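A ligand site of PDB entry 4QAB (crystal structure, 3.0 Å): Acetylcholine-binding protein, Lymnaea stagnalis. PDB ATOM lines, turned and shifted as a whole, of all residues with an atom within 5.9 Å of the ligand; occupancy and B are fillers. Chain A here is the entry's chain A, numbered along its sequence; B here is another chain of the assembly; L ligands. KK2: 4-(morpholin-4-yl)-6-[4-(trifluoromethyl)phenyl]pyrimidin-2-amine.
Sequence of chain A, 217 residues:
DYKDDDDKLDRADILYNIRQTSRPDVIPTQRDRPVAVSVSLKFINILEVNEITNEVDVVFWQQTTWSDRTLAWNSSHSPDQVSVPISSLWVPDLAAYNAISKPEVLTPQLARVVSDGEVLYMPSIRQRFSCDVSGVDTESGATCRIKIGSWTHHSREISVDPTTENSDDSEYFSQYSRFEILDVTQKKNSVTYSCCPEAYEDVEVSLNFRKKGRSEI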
ATOM      1  N   TYR A  97     -18.093  17.248  25.587  1.00  0.00           N
ATOM      2  CA  TYR A  97     -18.522  17.581  24.227  1.00  0.00           C
ATOM      3  C   TYR A  97     -19.743  18.518  24.157  1.00  0.00           C
ATOM      4  O   TYR A  97     -19.946  19.218  23.170  1.00  0.00           O
ATOM      5  CB  TYR A  97     -18.834  16.307  23.407  1.00  0.00           C
ATOM      6  CG  TYR A  97     -17.746  15.248  23.283  1.00  0.00           C
ATOM      7  CD1 TYR A  97     -18.075  13.995  22.808  1.00  0.00           C
ATOM      8  CD2 TYR A  97     -16.415  15.496  23.642  1.00  0.00           C
ATOM      9  CE1 TYR A  97     -17.123  12.995  22.674  1.00  0.00           C
ATOM     10  CE2 TYR A  97     -15.453  14.490  23.516  1.00  0.00           C
ATOM     11  CZ  TYR A  97     -15.823  13.237  23.031  1.00  0.00           C
ATOM     12  OH  TYR A  97     -14.914  12.210  22.892  1.00  0.00           O
ATOM     13  N   GLY A 149     -14.747  13.141  27.002  1.00  0.00           N
ATOM     14  CA  GLY A 149     -13.818  12.369  26.195  1.00  0.00           C
ATOM     15  C   GLY A 149     -12.386  12.877  26.199  1.00  0.00           C
ATOM     16  O   GLY A 149     -12.111  13.963  26.686  1.00  0.00           O
ATOM     17  N   SER A 150     -11.485  12.069  25.642  1.00  0.00           N
ATOM     18  CA  SER A 150     -10.133  12.552  25.382  1.00  0.00           C
ATOM     19  C   SER A 150     -10.152  13.372  24.113  1.00  0.00           C
ATOM     20  O   SER A 150     -10.562  12.879  23.057  1.00  0.00           O
ATOM     21  CB  SER A 150      -9.144  11.415  25.231  1.00  0.00           C
ATOM     22  OG  SER A 150      -7.878  11.930  24.826  1.00  0.00           O
ATOM     23  N   TRP A 151      -9.707  14.617  24.202  1.00  0.00           N
ATOM     24  CA  TRP A 151      -9.793  15.506  23.062  1.00  0.00           C
ATOM     25  C   TRP A 151      -8.864  15.083  21.932  1.00  0.00           C
ATOM     26  O   TRP A 151      -9.328  14.667  20.877  1.00  0.00           O
ATOM     27  CB  TRP A 151      -9.572  16.962  23.464  1.00  0.00           C
ATOM     28  CG  TRP A 151     -10.072  17.886  22.409  1.00  0.00           C
ATOM     29  CD1 TRP A 151      -9.346  18.781  21.680  1.00  0.00           C
ATOM     30  CD2 TRP A 151     -11.432  17.975  21.919  1.00  0.00           C
ATOM     31  NE1 TRP A 151     -10.162  19.429  20.783  1.00  0.00           N
ATOM     32  CE2 TRP A 151     -11.442  18.953  20.906  1.00  0.00           C
ATOM     33  CE3 TRP A 151     -12.623  17.329  22.253  1.00  0.00           C
ATOM     34  CZ2 TRP A 151     -12.602  19.296  20.221  1.00  0.00           C
ATOM     35  CZ3 TRP A 151     -13.773  17.671  21.567  1.00  0.00           C
ATOM     36  CH2 TRP A 151     -13.762  18.651  20.566  1.00  0.00           C
ATOM     37  N   THR A 152      -7.558  15.142  22.161  1.00  0.00           N
ATOM     38  CA  THR A 152      -6.610  14.915  21.073  1.00  0.00           C
ATOM     39  C   THR A 152      -6.041  13.507  21.002  1.00  0.00           C
ATOM     40  O   THR A 152      -5.419  13.160  20.018  1.00  0.00           O
ATOM     41  CB  THR A 152      -5.453  15.889  21.185  1.00  0.00           C
ATOM     42  OG1 THR A 152      -4.923  15.816  22.509  1.00  0.00           O
ATOM     43  CG2 THR A 152      -5.922  17.311  20.896  1.00  0.00           C
ATOM     44  N   HIS A 153      -6.226  12.707  22.036  1.00  0.00           N
ATOM     45  CA  HIS A 153      -5.725  11.335  21.977  1.00  0.00           C
ATOM     46  C   HIS A 153      -6.823  10.330  21.714  1.00  0.00           C
ATOM     47  O   HIS A 153      -7.877  10.354  22.354  1.00  0.00           O
ATOM     48  CB  HIS A 153      -4.982  10.962  23.262  1.00  0.00           C
ATOM     49  CG  HIS A 153      -3.803  11.836  23.547  1.00  0.00           C
ATOM     50  ND1 HIS A 153      -3.838  12.842  24.484  1.00  0.00           N
ATOM     51  CD2 HIS A 153      -2.568  11.868  22.989  1.00  0.00           C
ATOM     52  CE1 HIS A 153      -2.668  13.453  24.508  1.00  0.00           C
ATOM     53  NE2 HIS A 153      -1.878  12.883  23.617  1.00  0.00           N
ATOM     54  N   TYR A 193     -15.408   9.841  14.280  1.00  0.00           N
ATOM     55  CA  TYR A 193     -15.893  10.966  13.505  1.00  0.00           C
ATOM     56  C   TYR A 193     -15.260  10.919  12.120  1.00  0.00           C
ATOM     57  O   TYR A 193     -14.142  10.462  11.962  1.00  0.00           O
ATOM     58  CB  TYR A 193     -15.565  12.262  14.232  1.00  0.00           C
ATOM     59  CG  TYR A 193     -15.921  12.189  15.694  1.00  0.00           C
ATOM     60  CD1 TYR A 193     -17.195  12.507  16.120  1.00  0.00           C
ATOM     61  CD2 TYR A 193     -14.993  11.764  16.648  1.00  0.00           C
ATOM     62  CE1 TYR A 193     -17.541  12.419  17.453  1.00  0.00           C
ATOM     63  CE2 TYR A 193     -15.329  11.675  17.981  1.00  0.00           C
ATOM     64  CZ  TYR A 193     -16.613  12.016  18.374  1.00  0.00           C
ATOM     65  OH  TYR A 193     -16.990  11.927  19.695  1.00  0.00           O
ATOM     66  N   CYS A 195     -13.791  12.931  10.330  1.00  0.00           N
ATOM     67  CA  CYS A 195     -12.506  13.609  10.170  1.00  0.00           C
ATOM     68  C   CYS A 195     -11.309  12.625  10.245  1.00  0.00           C
ATOM     69  O   CYS A 195     -10.535  12.496   9.280  1.00  0.00           O
ATOM     70  CB  CYS A 195     -12.346  14.678  11.251  1.00  0.00           C
ATOM     71  SG  CYS A 195     -11.701  14.019  12.818  1.00  0.00           S
ATOM     72  N   CYS A 196     -11.166  11.939  11.372  1.00  0.00           N
ATOM     73  CA  CYS A 196      -9.993  11.106  11.663  1.00  0.00           C
ATOM     74  C   CYS A 196     -10.353   9.621  11.634  1.00  0.00           C
ATOM     75  O   CYS A 196     -11.378   9.221  12.206  1.00  0.00           O
ATOM     76  CB  CYS A 196      -9.433  11.458  13.043  1.00  0.00           C
ATOM     77  SG  CYS A 196     -10.133  13.014  13.695  1.00  0.00           S
ATOM     78  N   TYR A 200     -12.344   7.664  19.128  1.00  0.00           N
ATOM     79  CA  TYR A 200     -12.135   8.338  20.408  1.00  0.00           C
ATOM     80  C   TYR A 200     -13.005   7.794  21.550  1.00  0.00           C
ATOM     81  O   TYR A 200     -14.226   7.722  21.419  1.00  0.00           O
ATOM     82  CB  TYR A 200     -12.327   9.843  20.252  1.00  0.00           C
ATOM     83  CG  TYR A 200     -11.291  10.480  19.381  1.00  0.00           C
ATOM     84  CD1 TYR A 200     -11.385  10.406  17.996  1.00  0.00           C
ATOM     85  CD2 TYR A 200     -10.205  11.123  19.935  1.00  0.00           C
ATOM     86  CE1 TYR A 200     -10.421  10.971  17.197  1.00  0.00           C
ATOM     87  CE2 TYR A 200      -9.242  11.687  19.136  1.00  0.00           C
ATOM     88  CZ  TYR A 200      -9.364  11.614  17.775  1.00  0.00           C
ATOM     89  OH  TYR A 200      -8.399  12.181  16.990  1.00  0.00           O
ATOM     90  N   GLU A 201     -12.364   7.425  22.661  1.00  0.00           N
ATOM     91  CA  GLU A 201     -13.117   6.936  23.826  1.00  0.00           C
ATOM     92  C   GLU A 201     -13.724   8.078  24.605  1.00  0.00           C
ATOM     93  O   GLU A 201     -13.215   9.194  24.622  1.00  0.00           O
ATOM     94  CB  GLU A 201     -12.251   6.047  24.735  1.00  0.00           C
ATOM     95  CG  GLU A 201     -11.790   4.767  24.071  1.00  0.00           C
ATOM     96  CD  GLU A 201     -11.565   3.622  25.060  1.00  0.00           C
ATOM     97  OE1 GLU A 201     -11.918   3.793  26.250  1.00  0.00           O
ATOM     98  OE2 GLU A 201     -11.040   2.546  24.644  1.00  0.00           O
ATOM     99  N   ILE B  44     -21.792  23.210  16.159  1.00  0.00           N
ATOM    100  CA  ILE B  44     -22.101  22.309  17.284  1.00  0.00           C
ATOM    101  C   ILE B  44     -23.412  22.725  17.938  1.00  0.00           C
ATOM    102  O   ILE B  44     -24.202  21.886  18.347  1.00  0.00           O
ATOM    103  CB  ILE B  44     -20.992  22.353  18.382  1.00  0.00           C
ATOM    104  CG1 ILE B  44     -19.621  21.995  17.811  1.00  0.00           C
ATOM    105  CG2 ILE B  44     -21.308  21.394  19.468  1.00  0.00           C
ATOM    106  CD1 ILE B  44     -19.533  20.596  17.276  1.00  0.00           C
ATOM    107  N   TRP B  61     -16.940  23.896  15.786  1.00  0.00           N
ATOM    108  CA  TRP B  61     -15.708  23.132  15.788  1.00  0.00           C
ATOM    109  C   TRP B  61     -14.847  23.590  14.614  1.00  0.00           C
ATOM    110  O   TRP B  61     -15.184  23.330  13.457  1.00  0.00           O
ATOM    111  CB  TRP B  61     -16.005  21.647  15.652  1.00  0.00           C
ATOM    112  CG  TRP B  61     -14.794  20.812  15.752  1.00  0.00           C
ATOM    113  CD1 TRP B  61     -13.630  21.128  16.393  1.00  0.00           C
ATOM    114  CD2 TRP B  61     -14.598  19.518  15.200  1.00  0.00           C
ATOM    115  NE1 TRP B  61     -12.730  20.105  16.269  1.00  0.00           N
ATOM    116  CE2 TRP B  61     -13.306  19.100  15.528  1.00  0.00           C
ATOM    117  CE3 TRP B  61     -15.413  18.663  14.438  1.00  0.00           C
ATOM    118  CZ2 TRP B  61     -12.792  17.877  15.137  1.00  0.00           C
ATOM    119  CZ3 TRP B  61     -14.899  17.435  14.056  1.00  0.00           C
ATOM    120  CH2 TRP B  61     -13.602  17.064  14.402  1.00  0.00           C
ATOM    121  N   GLN B  81       1.892  10.107  14.913  1.00  0.00           N
ATOM    122  CA  GLN B  81       1.356  11.381  15.359  1.00  0.00           C
ATOM    123  C   GLN B  81       1.694  11.561  16.810  1.00  0.00           C
ATOM    124  O   GLN B  81       1.806  10.583  17.539  1.00  0.00           O
ATOM    125  CB  GLN B  81      -0.174  11.457  15.243  1.00  0.00           C
ATOM    126  CG  GLN B  81      -0.772  11.245  13.856  1.00  0.00           C
ATOM    127  CD  GLN B  81      -2.279  10.986  13.906  1.00  0.00           C
ATOM    128  OE1 GLN B  81      -3.030  11.723  14.546  1.00  0.00           O
ATOM    129  NE2 GLN B  81      -2.714   9.940  13.220  1.00  0.00           N
ATOM    130  N   LEU B 110      -4.154  21.943  22.368  1.00  0.00           N
ATOM    131  CA  LEU B 110      -3.160  21.046  21.802  1.00  0.00           C
ATOM    132  C   LEU B 110      -3.364  20.817  20.307  1.00  0.00           C
ATOM    133  O   LEU B 110      -4.492  20.797  19.830  1.00  0.00           O
ATOM    134  CB  LEU B 110      -3.204  19.685  22.490  1.00  0.00           C
ATOM    135  CG  LEU B 110      -3.081  19.657  24.011  1.00  0.00           C
ATOM    136  CD1 LEU B 110      -3.157  18.232  24.433  1.00  0.00           C
ATOM    137  CD2 LEU B 110      -1.792  20.278  24.466  1.00  0.00           C
ATOM    138  N   ALA B 111      -2.268  20.629  19.598  1.00  0.00           N
ATOM    139  CA  ALA B 111      -2.327  20.279  18.191  1.00  0.00           C
ATOM    140  C   ALA B 111      -1.788  18.864  17.986  1.00  0.00           C
ATOM    141  O   ALA B 111      -1.106  18.326  18.848  1.00  0.00           O
ATOM    142  CB  ALA B 111      -1.537  21.254  17.418  1.00  0.00           C
ATOM    143  N   ARG B 112      -2.122  18.254  16.855  1.00  0.00           N
ATOM    144  CA  ARG B 112      -1.469  17.009  16.472  1.00  0.00           C
ATOM    145  C   ARG B 112      -0.399  17.339  15.441  1.00  0.00           C
ATOM    146  O   ARG B 112      -0.581  18.190  14.586  1.00  0.00           O
ATOM    147  CB  ARG B 112      -2.447  16.024  15.854  1.00  0.00           C
ATOM    148  CG  ARG B 112      -3.516  15.542  16.789  1.00  0.00           C
ATOM    149  CD  ARG B 112      -2.960  14.653  17.890  1.00  0.00           C
ATOM    150  NE  ARG B 112      -2.766  13.278  17.429  1.00  0.00           N
ATOM    151  CZ  ARG B 112      -2.390  12.280  18.213  1.00  0.00           C
ATOM    152  NH1 ARG B 112      -2.169  12.505  19.504  1.00  0.00           N
ATOM    153  NH2 ARG B 112      -2.233  11.069  17.726  1.00  0.00           N
ATOM    154  N   LEU B 120      -2.365  19.658  12.665  1.00  0.00           N
ATOM    155  CA  LEU B 120      -3.800  19.830  12.810  1.00  0.00           C
ATOM    156  C   LEU B 120      -4.070  20.517  14.126  1.00  0.00           C
ATOM    157  O   LEU B 120      -3.536  20.136  15.147  1.00  0.00           O
ATOM    158  CB  LEU B 120      -4.532  18.490  12.758  1.00  0.00           C
ATOM    159  CG  LEU B 120      -4.019  17.486  11.724  1.00  0.00           C
ATOM    160  CD1 LEU B 120      -4.892  16.258  11.674  1.00  0.00           C
ATOM    161  CD2 LEU B 120      -3.952  18.100  10.349  1.00  0.00           C
ATOM    162  N   TYR B 121      -4.856  21.588  14.078  1.00  0.00           N
ATOM    163  CA  TYR B 121      -5.305  22.263  15.281  1.00  0.00           C
ATOM    164  C   TYR B 121      -6.804  22.467  15.163  1.00  0.00           C
ATOM    165  O   TYR B 121      -7.265  23.288  14.373  1.00  0.00           O
ATOM    166  CB  TYR B 121      -4.616  23.603  15.453  1.00  0.00           C
ATOM    167  CG  TYR B 121      -5.027  24.332  16.713  1.00  0.00           C
ATOM    168  CD1 TYR B 121      -5.245  23.634  17.894  1.00  0.00           C
ATOM    169  CD2 TYR B 121      -5.180  25.699  16.730  1.00  0.00           C
ATOM    170  CE1 TYR B 121      -5.607  24.300  19.056  1.00  0.00           C
ATOM    171  CE2 TYR B 121      -5.543  26.370  17.883  1.00  0.00           C
ATOM    172  CZ  TYR B 121      -5.761  25.674  19.042  1.00  0.00           C
ATOM    173  OH  TYR B 121      -6.124  26.351  20.186  1.00  0.00           O
ATOM    174  N   MET B 122      -7.564  21.710  15.944  1.00  0.00           N
ATOM    175  CA  MET B 122      -9.012  21.684  15.821  1.00  0.00           C
ATOM    176  C   MET B 122      -9.730  21.956  17.149  1.00  0.00           C
ATOM    177  O   MET B 122     -10.323  21.052  17.752  1.00  0.00           O
ATOM    178  CB  MET B 122      -9.427  20.343  15.220  1.00  0.00           C
ATOM    179  CG  MET B 122      -8.820  20.099  13.851  1.00  0.00           C
ATOM    180  SD  MET B 122      -9.147  18.496  13.083  1.00  0.00           S
ATOM    181  CE  MET B 122      -8.491  18.795  11.431  1.00  0.00           C
ATOM    182  N   TYR B 172     -22.436  17.020  13.746  1.00  0.00           N
ATOM    183  CA  TYR B 172     -21.958  17.270  15.098  1.00  0.00           C
ATOM    184  C   TYR B 172     -22.833  18.304  15.763  1.00  0.00           C
ATOM    185  O   TYR B 172     -22.469  18.853  16.796  1.00  0.00           O
ATOM    186  CB  TYR B 172     -20.535  17.798  15.090  1.00  0.00           C
ATOM    187  CG  TYR B 172     -19.558  17.040  14.233  1.00  0.00           C
ATOM    188  CD1 TYR B 172     -19.100  15.783  14.603  1.00  0.00           C
ATOM    189  CD2 TYR B 172     -19.060  17.593  13.076  1.00  0.00           C
ATOM    190  CE1 TYR B 172     -18.192  15.105  13.821  1.00  0.00           C
ATOM    191  CE2 TYR B 172     -18.151  16.929  12.291  1.00  0.00           C
ATOM    192  CZ  TYR B 172     -17.712  15.681  12.667  1.00  0.00           C
ATOM    193  OH  TYR B 172     -16.804  15.014  11.868  1.00  0.00           O
HETATM  194  C1  KK2 L   1     -16.090  16.111  17.241  1.00  0.00           C
HETATM  195  C2  KK2 L   1     -16.712  17.476  17.485  1.00  0.00           C
HETATM  196  O1  KK2 L   1     -17.933  17.303  18.132  1.00  0.00           O
HETATM  197  C3  KK2 L   1     -17.792  16.735  19.393  1.00  0.00           C
HETATM  198  C4  KK2 L   1     -17.050  15.370  19.313  1.00  0.00           C
HETATM  199  N2  KK2 L   1     -15.840  15.428  18.475  1.00  0.00           N
HETATM  200  C6  KK2 L   1     -14.472  15.176  18.825  1.00  0.00           C
HETATM  201  C5  KK2 L   1     -13.357  15.687  18.099  1.00  0.00           C
HETATM  202  N1  KK2 L   1     -14.269  14.387  19.934  1.00  0.00           N
HETATM  203  C7  KK2 L   1     -12.951  14.156  20.262  1.00  0.00           C
HETATM  204  N4  KK2 L   1     -12.726  13.393  21.363  1.00  0.00           N
HETATM  205  N3  KK2 L   1     -11.867  14.603  19.625  1.00  0.00           N
HETATM  206  C8  KK2 L   1     -12.071  15.358  18.531  1.00  0.00           C
HETATM  207  C9  KK2 L   1     -10.824  15.795  17.933  1.00  0.00           C
HETATM  208  C10 KK2 L   1     -10.135  16.937  18.381  1.00  0.00           C
HETATM  209  C11 KK2 L   1      -8.908  17.329  17.838  1.00  0.00           C
HETATM  210  C12 KK2 L   1      -8.311  16.580  16.836  1.00  0.00           C
HETATM  211  C13 KK2 L   1      -6.992  17.025  16.267  1.00  0.00           C
HETATM  212  F1  KK2 L   1      -6.138  17.494  17.198  1.00  0.00           F
HETATM  213  F2  KK2 L   1      -7.075  18.009  15.353  1.00  0.00           F
HETATM  214  F3  KK2 L   1      -6.325  16.039  15.587  1.00  0.00           F
HETATM  215  C14 KK2 L   1      -8.952  15.420  16.388  1.00  0.00           C
HETATM  216  C15 KK2 L   1     -10.178  15.036  16.936  1.00  0.00           C
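A nitrogen (N3) of the ligand lies close to the backbone carbonyl oxygen (O) of Trp 151 (2.8 Å). SD of Met 122 of chain B lies close to F2 of the ligand (3.1 Å). Thr 152 touches the ligand. Tyr 193 touches the ligand (OH to C4, 3.5 Å). Cys 196 touches the ligand. Tyr 200 touches the ligand (OH to C14, 3.3 Å). CD1 of Ile 44 of chain B touches O1 of the ligand, 3.8 Å away. Trp 61 of chain B touches the ligand (CE3 to C2, 3.5 Å). Arg 112 of chain B touches the ligand. Leu 120 of chain B touches the ligand (CB to F2, 3.7 Å). Hydrophobic or aromatic side chains that line the ligand: Tyr 97, Trp 151, Tyr 193, Tyr 200, Ile 44 of chain B, Trp 61 of chain B, Leu 120 of chain B and Met 122 of chain B. Within 4 Å of the ligand: Tyr 97, Ser 150, Trp 151, Thr 152, Tyr 193, Cys 196, Tyr 200, Ile 44 of chain B, Trp 61 of chain B, Arg 112 of chain B, Leu 120 of chain B and Met 122 of chain B. The nearest printed residue that does not touch the ligand is Tyr 172 of chain B (4.02 Å).
SG of Cys 195 is disulfide-bonded to SG of Cys 196 (2.1 Å). OE1 of Gln 81 of chain B lies within hydrogen-bond range of NE of Arg 112 of chain B (3.3 Å). The indole nitrogen (NE1) of Trp 151 is in hydrogen-bond range of the backbone carbonyl oxygen (O) of Met 122 of chain B (3.4 Å). OG of Ser 150 sits at hydrogen-bond distance from O of His 153 (2.9 Å). O of Thr 152 is in hydrogen-bond range of NH1 of Arg 112 of chain B (3.4 Å). The backbone NH (N) of Arg 112 of chain B sits at hydrogen-bond distance from the backbone carbonyl oxygen (O) of Leu 120 of chain B (2.9 Å). The backbone carbonyl oxygen of Met 122 of chain B sits at hydrogen-bond distance from the indole nitrogen of Trp 61 of chain B.
A nitrogen (N4) of the ligand sits at hydrogen-bond distance from the side-chain hydroxyl (OH) of Tyr 97 (2.9 Å). The backbone carbonyl oxygen (O) of Ser 150 lies within hydrogen-bond range of a nitrogen (N4) of the ligand (2.8 Å).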
